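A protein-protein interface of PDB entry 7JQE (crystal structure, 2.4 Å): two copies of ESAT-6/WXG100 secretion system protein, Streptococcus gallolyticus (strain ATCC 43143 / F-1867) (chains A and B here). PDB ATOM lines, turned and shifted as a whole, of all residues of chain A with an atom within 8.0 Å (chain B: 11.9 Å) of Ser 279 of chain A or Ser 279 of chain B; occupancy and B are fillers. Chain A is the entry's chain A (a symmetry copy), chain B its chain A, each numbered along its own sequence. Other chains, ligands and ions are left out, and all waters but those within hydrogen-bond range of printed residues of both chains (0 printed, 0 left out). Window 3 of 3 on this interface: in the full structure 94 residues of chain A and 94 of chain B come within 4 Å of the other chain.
The side-chain amide oxygen of Asn 382 of chain B lies within hydrogen-bond range of the backbone NH of Ala 276 of chain A, 2.6 Å away.
O of Thr 278 of chain B sits close to OD1 of Asp 325 of chain B, 2.7 Å away. The side-chain hydroxyl (OG1) of Thr 327 of chain B sits at hydrogen-bond distance from the backbone NH (N) of Thr 278 of chain B, at 3.2 Å. O of Thr 278 of chain A sits close to OD1 of Asp 325 of chain A (2.7 Å). N of Thr 278 of chain A sits at hydrogen-bond distance from OG1 of Thr 327 of chain A (3.2 Å).
Among the printed residues, pairs that only touch across the chains: Ser 279 of chain A with Thr 278 of chain B, Thr 278 of chain A with Ser 279 of chain B, Ser 279 of chain A with Ser 279 of chain B, Ala 276 of chain A with Asp 381 of chain B and Asp 381 of chain A with Ala 276 of chain B.
Of the printed residues of chain B, Ala 276 of chain A touches Asp 381 and Asn 382. Pro 277 of chain A touches none of the printed residues of chain B. Thr 278 of chain A touches just one residue of chain B: Ser 279. Of chain B, only Thr 278 (3.6 Å) and Ser 279 (3.7 Å) come within 4 Å of Ser 279 of chain A. No residue of chain B comes within 4 Å of Asp 325 of chain A. Printed residues of chain B within 4 Å of Asp 381 of chain A: Ala 276 (3.7 Å). Ser 279 of chain B touches just these residues of chain A: Thr 278 and Ser 279. Of the printed residues of chain A, Asp 381 of chain B touches Ala 276 (3.7 Å). Printed residues of chain A within 4 Å of Asn 382 of chain B: Ala 276. The nearest printed residue of chain A that does not touch Asn 382 of chain B is Pro 277 of chain A (5.4 Å).
Hydrophobic or aromatic side chains of chain A that line the printed part of chain B: Ala 276. Of the 20 printed residues of chain B, 5 touch a printed residue of chain A. Hydrophobic or aromatic side chains of chain B within 4 Å of the printed part of chain A: Ala 276. Among the printed residues, 6 pairs touch across the chains. Among the printed residues, no Asp or Glu carboxylate lies within 4 Å of a Lys or Arg side-chain nitrogen of the other chain.
Ala 276 of chain A touches Asp 381 of chain B, and with the chains exchanged Asp 381 of chain A touches Ala 276 of chain B. Thr 278 of chain A touches Ser 279 of chain B, and with the chains exchanged Ser 279 of chain A touches Thr 278 of chain B. Ser 279 of chain B touches its own counterpart, Ser 279 of chain A. Of the 6 pairs that touch across the chains among the printed residues, 5 have their exchanged pair printed and touching as well.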
ATOM      1  N   ALA A 276     -17.779 -11.719  13.634  1.00  0.00           N
ATOM      2  CA  ALA A 276     -18.984 -11.313  12.927  1.00  0.00           C
ATOM      3  C   ALA A 276     -20.146 -12.166  13.412  1.00  0.00           C
ATOM      4  O   ALA A 276     -19.965 -13.370  13.648  1.00  0.00           O
ATOM      5  CB  ALA A 276     -18.833 -11.452  11.409  1.00  0.00           C
ATOM      6  N   PRO A 277     -21.331 -11.585  13.572  1.00  0.00           N
ATOM      7  CA  PRO A 277     -22.483 -12.372  14.023  1.00  0.00           C
ATOM      8  C   PRO A 277     -22.890 -13.411  12.990  1.00  0.00           C
ATOM      9  O   PRO A 277     -22.518 -13.346  11.816  1.00  0.00           O
ATOM     10  CB  PRO A 277     -23.580 -11.318  14.215  1.00  0.00           C
ATOM     11  CG  PRO A 277     -23.185 -10.200  13.298  1.00  0.00           C
ATOM     12  CD  PRO A 277     -21.682 -10.177  13.322  1.00  0.00           C
ATOM     13  N   THR A 278     -23.662 -14.393  13.449  1.00  0.00           N
ATOM     14  CA  THR A 278     -24.224 -15.418  12.573  1.00  0.00           C
ATOM     15  C   THR A 278     -25.616 -14.966  12.141  1.00  0.00           C
ATOM     16  O   THR A 278     -26.537 -14.882  12.962  1.00  0.00           O
ATOM     17  CB  THR A 278     -24.279 -16.776  13.272  1.00  0.00           C
ATOM     18  OG1 THR A 278     -25.469 -16.867  14.064  1.00  0.00           O
ATOM     19  CG2 THR A 278     -23.060 -16.963  14.174  1.00  0.00           C
ATOM     20  N   SER A 279     -25.765 -14.668  10.854  1.00  0.00           N
ATOM     21  CA  SER A 279     -27.036 -14.211  10.303  1.00  0.00           C
ATOM     22  C   SER A 279     -28.192 -15.108  10.726  1.00  0.00           C
ATOM     23  O   SER A 279     -29.298 -15.006  10.186  1.00  0.00           O
ATOM     24  CB  SER A 279     -26.956 -14.147   8.775  1.00  0.00           C
ATOM     25  OG  SER A 279     -26.506 -15.380   8.233  1.00  0.00           O
ATOM     26  N   THR A 322     -32.837  -8.596   8.136  1.00  0.00           N
ATOM     27  CA  THR A 322     -31.746  -8.103   8.969  1.00  0.00           C
ATOM     28  C   THR A 322     -31.690  -8.878  10.281  1.00  0.00           C
ATOM     29  O   THR A 322     -31.324  -8.333  11.324  1.00  0.00           O
ATOM     30  CB  THR A 322     -31.894  -6.597   9.265  1.00  0.00           C
ATOM     31  OG1 THR A 322     -32.186  -5.895   8.050  1.00  0.00           O
ATOM     32  CG2 THR A 322     -30.609  -6.038   9.864  1.00  0.00           C
ATOM     33  N   LYS A 323     -32.058 -10.158  10.223  1.00  0.00           N
ATOM     34  CA  LYS A 323     -32.035 -11.027  11.399  1.00  0.00           C
ATOM     35  C   LYS A 323     -30.607 -11.506  11.689  1.00  0.00           C
ATOM     36  O   LYS A 323     -30.288 -12.693  11.640  1.00  0.00           O
ATOM     37  CB  LYS A 323     -32.987 -12.200  11.212  1.00  0.00           C
ATOM     38  CG  LYS A 323     -33.216 -12.607   9.765  1.00  0.00           C
ATOM     39  CD  LYS A 323     -34.354 -11.809   9.146  1.00  0.00           C
ATOM     40  CE  LYS A 323     -34.700 -12.306   7.748  1.00  0.00           C
ATOM     41  NZ  LYS A 323     -35.962 -11.686   7.235  1.00  0.00           N
ATOM     42  N   GLU A 324     -29.739 -10.537  11.991  1.00  0.00           N
ATOM     43  CA  GLU A 324     -28.367 -10.814  12.423  1.00  0.00           C
ATOM     44  C   GLU A 324     -28.354 -10.836  13.949  1.00  0.00           C
ATOM     45  O   GLU A 324     -28.037  -9.853  14.622  1.00  0.00           O
ATOM     46  CB  GLU A 324     -27.405  -9.777  11.860  1.00  0.00           C
ATOM     47  CG  GLU A 324     -27.849  -8.348  12.113  1.00  0.00           C
ATOM     48  CD  GLU A 324     -26.927  -7.330  11.478  1.00  0.00           C
ATOM     49  OE1 GLU A 324     -25.691  -7.512  11.554  1.00  0.00           O
ATOM     50  OE2 GLU A 324     -27.445  -6.353  10.895  1.00  0.00           O
ATOM     51  N   ASP A 325     -28.706 -11.996  14.495  1.00  0.00           N
ATOM     52  CA  ASP A 325     -28.963 -12.124  15.918  1.00  0.00           C
ATOM     53  C   ASP A 325     -27.688 -11.920  16.734  1.00  0.00           C
ATOM     54  O   ASP A 325     -26.575 -12.028  16.212  1.00  0.00           O
ATOM     55  CB  ASP A 325     -29.563 -13.494  16.220  1.00  0.00           C
ATOM     56  CG  ASP A 325     -29.851 -14.293  14.962  1.00  0.00           C
ATOM     57  OD1 ASP A 325     -28.885 -14.752  14.313  1.00  0.00           O
ATOM     58  OD2 ASP A 325     -31.042 -14.457  14.620  1.00  0.00           O
ATOM     59  N   THR A 327     -24.523 -12.629  18.965  1.00  0.00           N
ATOM     60  CA  THR A 327     -23.605 -13.761  18.968  1.00  0.00           C
ATOM     61  C   THR A 327     -22.559 -13.547  20.051  1.00  0.00           C
ATOM     62  O   THR A 327     -21.895 -12.506  20.080  1.00  0.00           O
ATOM     63  CB  THR A 327     -22.931 -13.936  17.603  1.00  0.00           C
ATOM     64  OG1 THR A 327     -23.911 -13.802  16.564  1.00  0.00           O
ATOM     65  CG2 THR A 327     -22.290 -15.308  17.504  1.00  0.00           C
ATOM     66  N   ASP A 381     -21.113 -21.318  17.657  1.00  0.00           N
ATOM     67  CA  ASP A 381     -20.830 -22.748  17.729  1.00  0.00           C
ATOM     68  C   ASP A 381     -19.434 -23.107  17.233  1.00  0.00           C
ATOM     69  O   ASP A 381     -19.084 -24.293  17.224  1.00  0.00           O
ATOM     70  CB  ASP A 381     -21.875 -23.536  16.930  1.00  0.00           C
ATOM     71  CG  ASP A 381     -23.215 -23.617  17.640  1.00  0.00           C
ATOM     72  OD1 ASP A 381     -23.228 -23.660  18.890  1.00  0.00           O
ATOM     73  OD2 ASP A 381     -24.254 -23.641  16.948  1.00  0.00           O
ATOM     74  N   VAL B 275     -16.020 -26.300  13.339  1.00  0.00           N
ATOM     75  CA  VAL B 275     -16.664 -25.287  12.520  1.00  0.00           C
ATOM     76  C   VAL B 275     -18.163 -25.552  12.487  1.00  0.00           C
ATOM     77  O   VAL B 275     -18.637 -26.664  12.739  1.00  0.00           O
ATOM     78  CB  VAL B 275     -16.079 -25.241  11.089  1.00  0.00           C
ATOM     79  CG1 VAL B 275     -14.599 -24.891  11.128  1.00  0.00           C
ATOM     80  CG2 VAL B 275     -16.306 -26.566  10.381  1.00  0.00           C
ATOM     81  N   ALA B 276     -18.927 -24.505  12.170  1.00  0.00           N
ATOM     82  CA  ALA B 276     -20.377 -24.583  12.091  1.00  0.00           C
ATOM     83  C   ALA B 276     -20.872 -23.526  11.117  1.00  0.00           C
ATOM     84  O   ALA B 276     -20.328 -22.411  11.095  1.00  0.00           O
ATOM     85  CB  ALA B 276     -21.037 -24.382  13.459  1.00  0.00           C
ATOM     86  N   PRO B 277     -21.881 -23.836  10.308  1.00  0.00           N
ATOM     87  CA  PRO B 277     -22.400 -22.841   9.363  1.00  0.00           C
ATOM     88  C   PRO B 277     -23.052 -21.671  10.084  1.00  0.00           C
ATOM     89  O   PRO B 277     -23.394 -21.741  11.267  1.00  0.00           O
ATOM     90  CB  PRO B 277     -23.426 -23.633   8.544  1.00  0.00           C
ATOM     91  CG  PRO B 277     -23.846 -24.748   9.453  1.00  0.00           C
ATOM     92  CD  PRO B 277     -22.616 -25.110  10.238  1.00  0.00           C
ATOM     93  N   THR B 278     -23.213 -20.574   9.348  1.00  0.00           N
ATOM     94  CA  THR B 278     -23.911 -19.393   9.851  1.00  0.00           C
ATOM     95  C   THR B 278     -25.377 -19.493   9.439  1.00  0.00           C
ATOM     96  O   THR B 278     -25.705 -19.422   8.248  1.00  0.00           O
ATOM     97  CB  THR B 278     -23.276 -18.108   9.324  1.00  0.00           C
ATOM     98  OG1 THR B 278     -23.800 -17.804   8.025  1.00  0.00           O
ATOM     99  CG2 THR B 278     -21.760 -18.259   9.231  1.00  0.00           C
ATOM    100  N   SER B 279     -26.255 -19.663  10.422  1.00  0.00           N
ATOM    101  CA  SER B 279     -27.688 -19.785  10.174  1.00  0.00           C
ATOM    102  C   SER B 279     -28.200 -18.683   9.258  1.00  0.00           C
ATOM    103  O   SER B 279     -29.412 -18.498   9.113  1.00  0.00           O
ATOM    104  CB  SER B 279     -28.455 -19.764  11.498  1.00  0.00           C
ATOM    105  OG  SER B 279     -28.104 -18.632  12.278  1.00  0.00           O
ATOM    106  N   THR B 322     -34.829 -23.802   8.515  1.00  0.00           N
ATOM    107  CA  THR B 322     -33.605 -24.580   8.366  1.00  0.00           C
ATOM    108  C   THR B 322     -32.682 -23.927   7.344  1.00  0.00           C
ATOM    109  O   THR B 322     -31.948 -24.608   6.626  1.00  0.00           O
ATOM    110  CB  THR B 322     -33.905 -26.032   7.938  1.00  0.00           C
ATOM    111  OG1 THR B 322     -34.951 -26.567   8.758  1.00  0.00           O
ATOM    112  CG2 THR B 322     -32.663 -26.903   8.086  1.00  0.00           C
ATOM    113  N   LYS B 323     -32.726 -22.595   7.280  1.00  0.00           N
ATOM    114  CA  LYS B 323     -31.881 -21.835   6.361  1.00  0.00           C
ATOM    115  C   LYS B 323     -30.457 -21.708   6.914  1.00  0.00           C
ATOM    116  O   LYS B 323     -29.957 -20.621   7.204  1.00  0.00           O
ATOM    117  CB  LYS B 323     -32.494 -20.467   6.085  1.00  0.00           C
ATOM    118  CG  LYS B 323     -33.364 -19.924   7.207  1.00  0.00           C
ATOM    119  CD  LYS B 323     -34.801 -20.404   7.065  1.00  0.00           C
ATOM    120  CE  LYS B 323     -35.722 -19.751   8.089  1.00  0.00           C
ATOM    121  NZ  LYS B 323     -37.162 -20.036   7.802  1.00  0.00           N
ATOM    122  N   GLU B 324     -29.806 -22.865   7.061  1.00  0.00           N
ATOM    123  CA  GLU B 324     -28.395 -22.931   7.452  1.00  0.00           C
ATOM    124  C   GLU B 324     -27.562 -23.014   6.176  1.00  0.00           C
ATOM    125  O   GLU B 324     -27.163 -24.085   5.714  1.00  0.00           O
ATOM    126  CB  GLU B 324     -28.147 -24.117   8.372  1.00  0.00           C
ATOM    127  CG  GLU B 324     -28.692 -25.424   7.827  1.00  0.00           C
ATOM    128  CD  GLU B 324     -28.511 -26.578   8.788  1.00  0.00           C
ATOM    129  OE1 GLU B 324     -27.424 -26.684   9.398  1.00  0.00           O
ATOM    130  OE2 GLU B 324     -29.465 -27.375   8.936  1.00  0.00           O
ATOM    131  N   ASP B 325     -27.295 -21.842   5.604  1.00  0.00           N
ATOM    132  CA  ASP B 325     -26.713 -21.756   4.277  1.00  0.00           C
ATOM    133  C   ASP B 325     -25.283 -22.293   4.261  1.00  0.00           C
ATOM    134  O   ASP B 325     -24.633 -22.404   5.304  1.00  0.00           O
ATOM    135  CB  ASP B 325     -26.732 -20.308   3.792  1.00  0.00           C
ATOM    136  CG  ASP B 325     -27.461 -19.384   4.750  1.00  0.00           C
ATOM    137  OD1 ASP B 325     -26.920 -19.111   5.844  1.00  0.00           O
ATOM    138  OD2 ASP B 325     -28.577 -18.935   4.410  1.00  0.00           O
ATOM    139  N   PRO B 326     -24.777 -22.643   3.080  1.00  0.00           N
ATOM    140  CA  PRO B 326     -23.385 -23.095   2.979  1.00  0.00           C
ATOM    141  C   PRO B 326     -22.417 -22.021   3.458  1.00  0.00           C
ATOM    142  O   PRO B 326     -22.619 -20.827   3.228  1.00  0.00           O
ATOM    143  CB  PRO B 326     -23.213 -23.384   1.484  1.00  0.00           C
ATOM    144  CG  PRO B 326     -24.608 -23.647   0.987  1.00  0.00           C
ATOM    145  CD  PRO B 326     -25.500 -22.759   1.800  1.00  0.00           C
ATOM    146  N   THR B 327     -21.352 -22.462   4.128  1.00  0.00           N
ATOM    147  CA  THR B 327     -20.350 -21.567   4.692  1.00  0.00           C
ATOM    148  C   THR B 327     -18.966 -22.083   4.328  1.00  0.00           C
ATOM    149  O   THR B 327     -18.644 -23.246   4.590  1.00  0.00           O
ATOM    150  CB  THR B 327     -20.494 -21.457   6.213  1.00  0.00           C
ATOM    151  OG1 THR B 327     -21.879 -21.301   6.554  1.00  0.00           O
ATOM    152  CG2 THR B 327     -19.718 -20.261   6.732  1.00  0.00           C
ATOM    153  N   THR B 328     -18.153 -21.216   3.727  1.00  0.00           N
ATOM    154  CA  THR B 328     -16.856 -21.598   3.184  1.00  0.00           C
ATOM    155  C   THR B 328     -15.755 -21.269   4.188  1.00  0.00           C
ATOM    156  O   THR B 328     -15.629 -20.123   4.630  1.00  0.00           O
ATOM    157  CB  THR B 328     -16.601 -20.892   1.852  1.00  0.00           C
ATOM    158  OG1 THR B 328     -16.569 -19.474   2.060  1.00  0.00           O
ATOM    159  CG2 THR B 328     -17.706 -21.227   0.852  1.00  0.00           C
ATOM    160  N   ILE B 351     -18.996 -25.919   4.089  1.00  0.00           N
ATOM    161  CA  ILE B 351     -19.754 -26.827   4.935  1.00  0.00           C
ATOM    162  C   ILE B 351     -21.206 -26.359   4.999  1.00  0.00           C
ATOM    163  O   ILE B 351     -21.544 -25.240   4.609  1.00  0.00           O
ATOM    164  CB  ILE B 351     -19.158 -26.936   6.350  1.00  0.00           C
ATOM    165  CG1 ILE B 351     -19.252 -25.587   7.063  1.00  0.00           C
ATOM    166  CG2 ILE B 351     -17.711 -27.398   6.282  1.00  0.00           C
ATOM    167  CD1 ILE B 351     -18.718 -25.606   8.476  1.00  0.00           C
ATOM    168  N   SER B 352     -22.073 -27.249   5.502  1.00  0.00           N
ATOM    169  CA  SER B 352     -23.459 -26.890   5.783  1.00  0.00           C
ATOM    170  C   SER B 352     -23.949 -27.493   7.096  1.00  0.00           C
ATOM    171  O   SER B 352     -25.166 -27.584   7.308  1.00  0.00           O
ATOM    172  CB  SER B 352     -24.394 -27.322   4.643  1.00  0.00           C
ATOM    173  OG  SER B 352     -24.148 -26.572   3.466  1.00  0.00           O
ATOM    174  N   LYS B 353     -23.041 -27.903   7.979  1.00  0.00           N
ATOM    175  CA  LYS B 353     -23.425 -28.501   9.250  1.00  0.00           C
ATOM    176  C   LYS B 353     -22.236 -28.466  10.200  1.00  0.00           C
ATOM    177  O   LYS B 353     -21.082 -28.426   9.766  1.00  0.00           O
ATOM    178  CB  LYS B 353     -23.919 -29.940   9.056  1.00  0.00           C
ATOM    179  CG  LYS B 353     -24.330 -30.622  10.343  1.00  0.00           C
ATOM    180  CD  LYS B 353     -25.300 -29.756  11.130  1.00  0.00           C
ATOM    181  CE  LYS B 353     -25.583 -30.355  12.496  1.00  0.00           C
ATOM    182  NZ  LYS B 353     -26.438 -29.463  13.322  1.00  0.00           N
ATOM    183  N   ALA B 354     -22.533 -28.477  11.501  1.00  0.00           N
ATOM    184  CA  ALA B 354     -21.482 -28.527  12.510  1.00  0.00           C
ATOM    185  C   ALA B 354     -20.559 -29.707  12.244  1.00  0.00           C
ATOM    186  O   ALA B 354     -21.009 -30.799  11.886  1.00  0.00           O
ATOM    187  CB  ALA B 354     -22.091 -28.632  13.911  1.00  0.00           C
ATOM    188  N   ILE B 379     -13.573 -18.471   8.748  1.00  0.00           N
ATOM    189  CA  ILE B 379     -14.856 -19.163   8.830  1.00  0.00           C
ATOM    190  C   ILE B 379     -15.919 -18.107   8.565  1.00  0.00           C
ATOM    191  O   ILE B 379     -16.242 -17.309   9.453  1.00  0.00           O
ATOM    192  CB  ILE B 379     -15.076 -19.840  10.186  1.00  0.00           C
ATOM    193  CG1 ILE B 379     -13.918 -20.788  10.512  1.00  0.00           C
ATOM    194  CG2 ILE B 379     -16.423 -20.568  10.202  1.00  0.00           C
ATOM    195  CD1 ILE B 379     -14.000 -21.401  11.892  1.00  0.00           C
ATOM    196  N   GLY B 380     -16.463 -18.092   7.351  1.00  0.00           N
ATOM    197  CA  GLY B 380     -17.376 -17.021   6.993  1.00  0.00           C
ATOM    198  C   GLY B 380     -16.665 -15.683   7.041  1.00  0.00           C
ATOM    199  O   GLY B 380     -15.532 -15.535   6.565  1.00  0.00           O
ATOM    200  N   ASP B 381     -17.330 -14.691   7.633  1.00  0.00           N
ATOM    201  CA  ASP B 381     -16.741 -13.370   7.819  1.00  0.00           C
ATOM    202  C   ASP B 381     -15.791 -13.301   9.009  1.00  0.00           C
ATOM    203  O   ASP B 381     -15.245 -12.226   9.282  1.00  0.00           O
ATOM    204  CB  ASP B 381     -17.843 -12.316   7.983  1.00  0.00           C
ATOM    205  CG  ASP B 381     -18.535 -11.985   6.673  1.00  0.00           C
ATOM    206  OD1 ASP B 381     -17.866 -12.022   5.616  1.00  0.00           O
ATOM    207  OD2 ASP B 381     -19.746 -11.682   6.699  1.00  0.00           O
ATOM    208  N   ASN B 382     -15.579 -14.411   9.715  1.00  0.00           N
ATOM    209  CA  ASN B 382     -14.655 -14.461  10.842  1.00  0.00           C
ATOM    210  C   ASN B 382     -13.249 -14.787  10.348  1.00  0.00           C
ATOM    211  O   ASN B 382     -13.065 -15.719   9.559  1.00  0.00           O
ATOM    212  CB  ASN B 382     -15.111 -15.508  11.861  1.00  0.00           C
ATOM    213  CG  ASN B 382     -16.289 -15.043  12.693  1.00  0.00           C
ATOM    214  OD1 ASN B 382     -16.416 -13.861  13.008  1.00  0.00           O
ATOM    215  ND2 ASN B 382     -17.155 -15.978  13.061  1.00  0.00           N
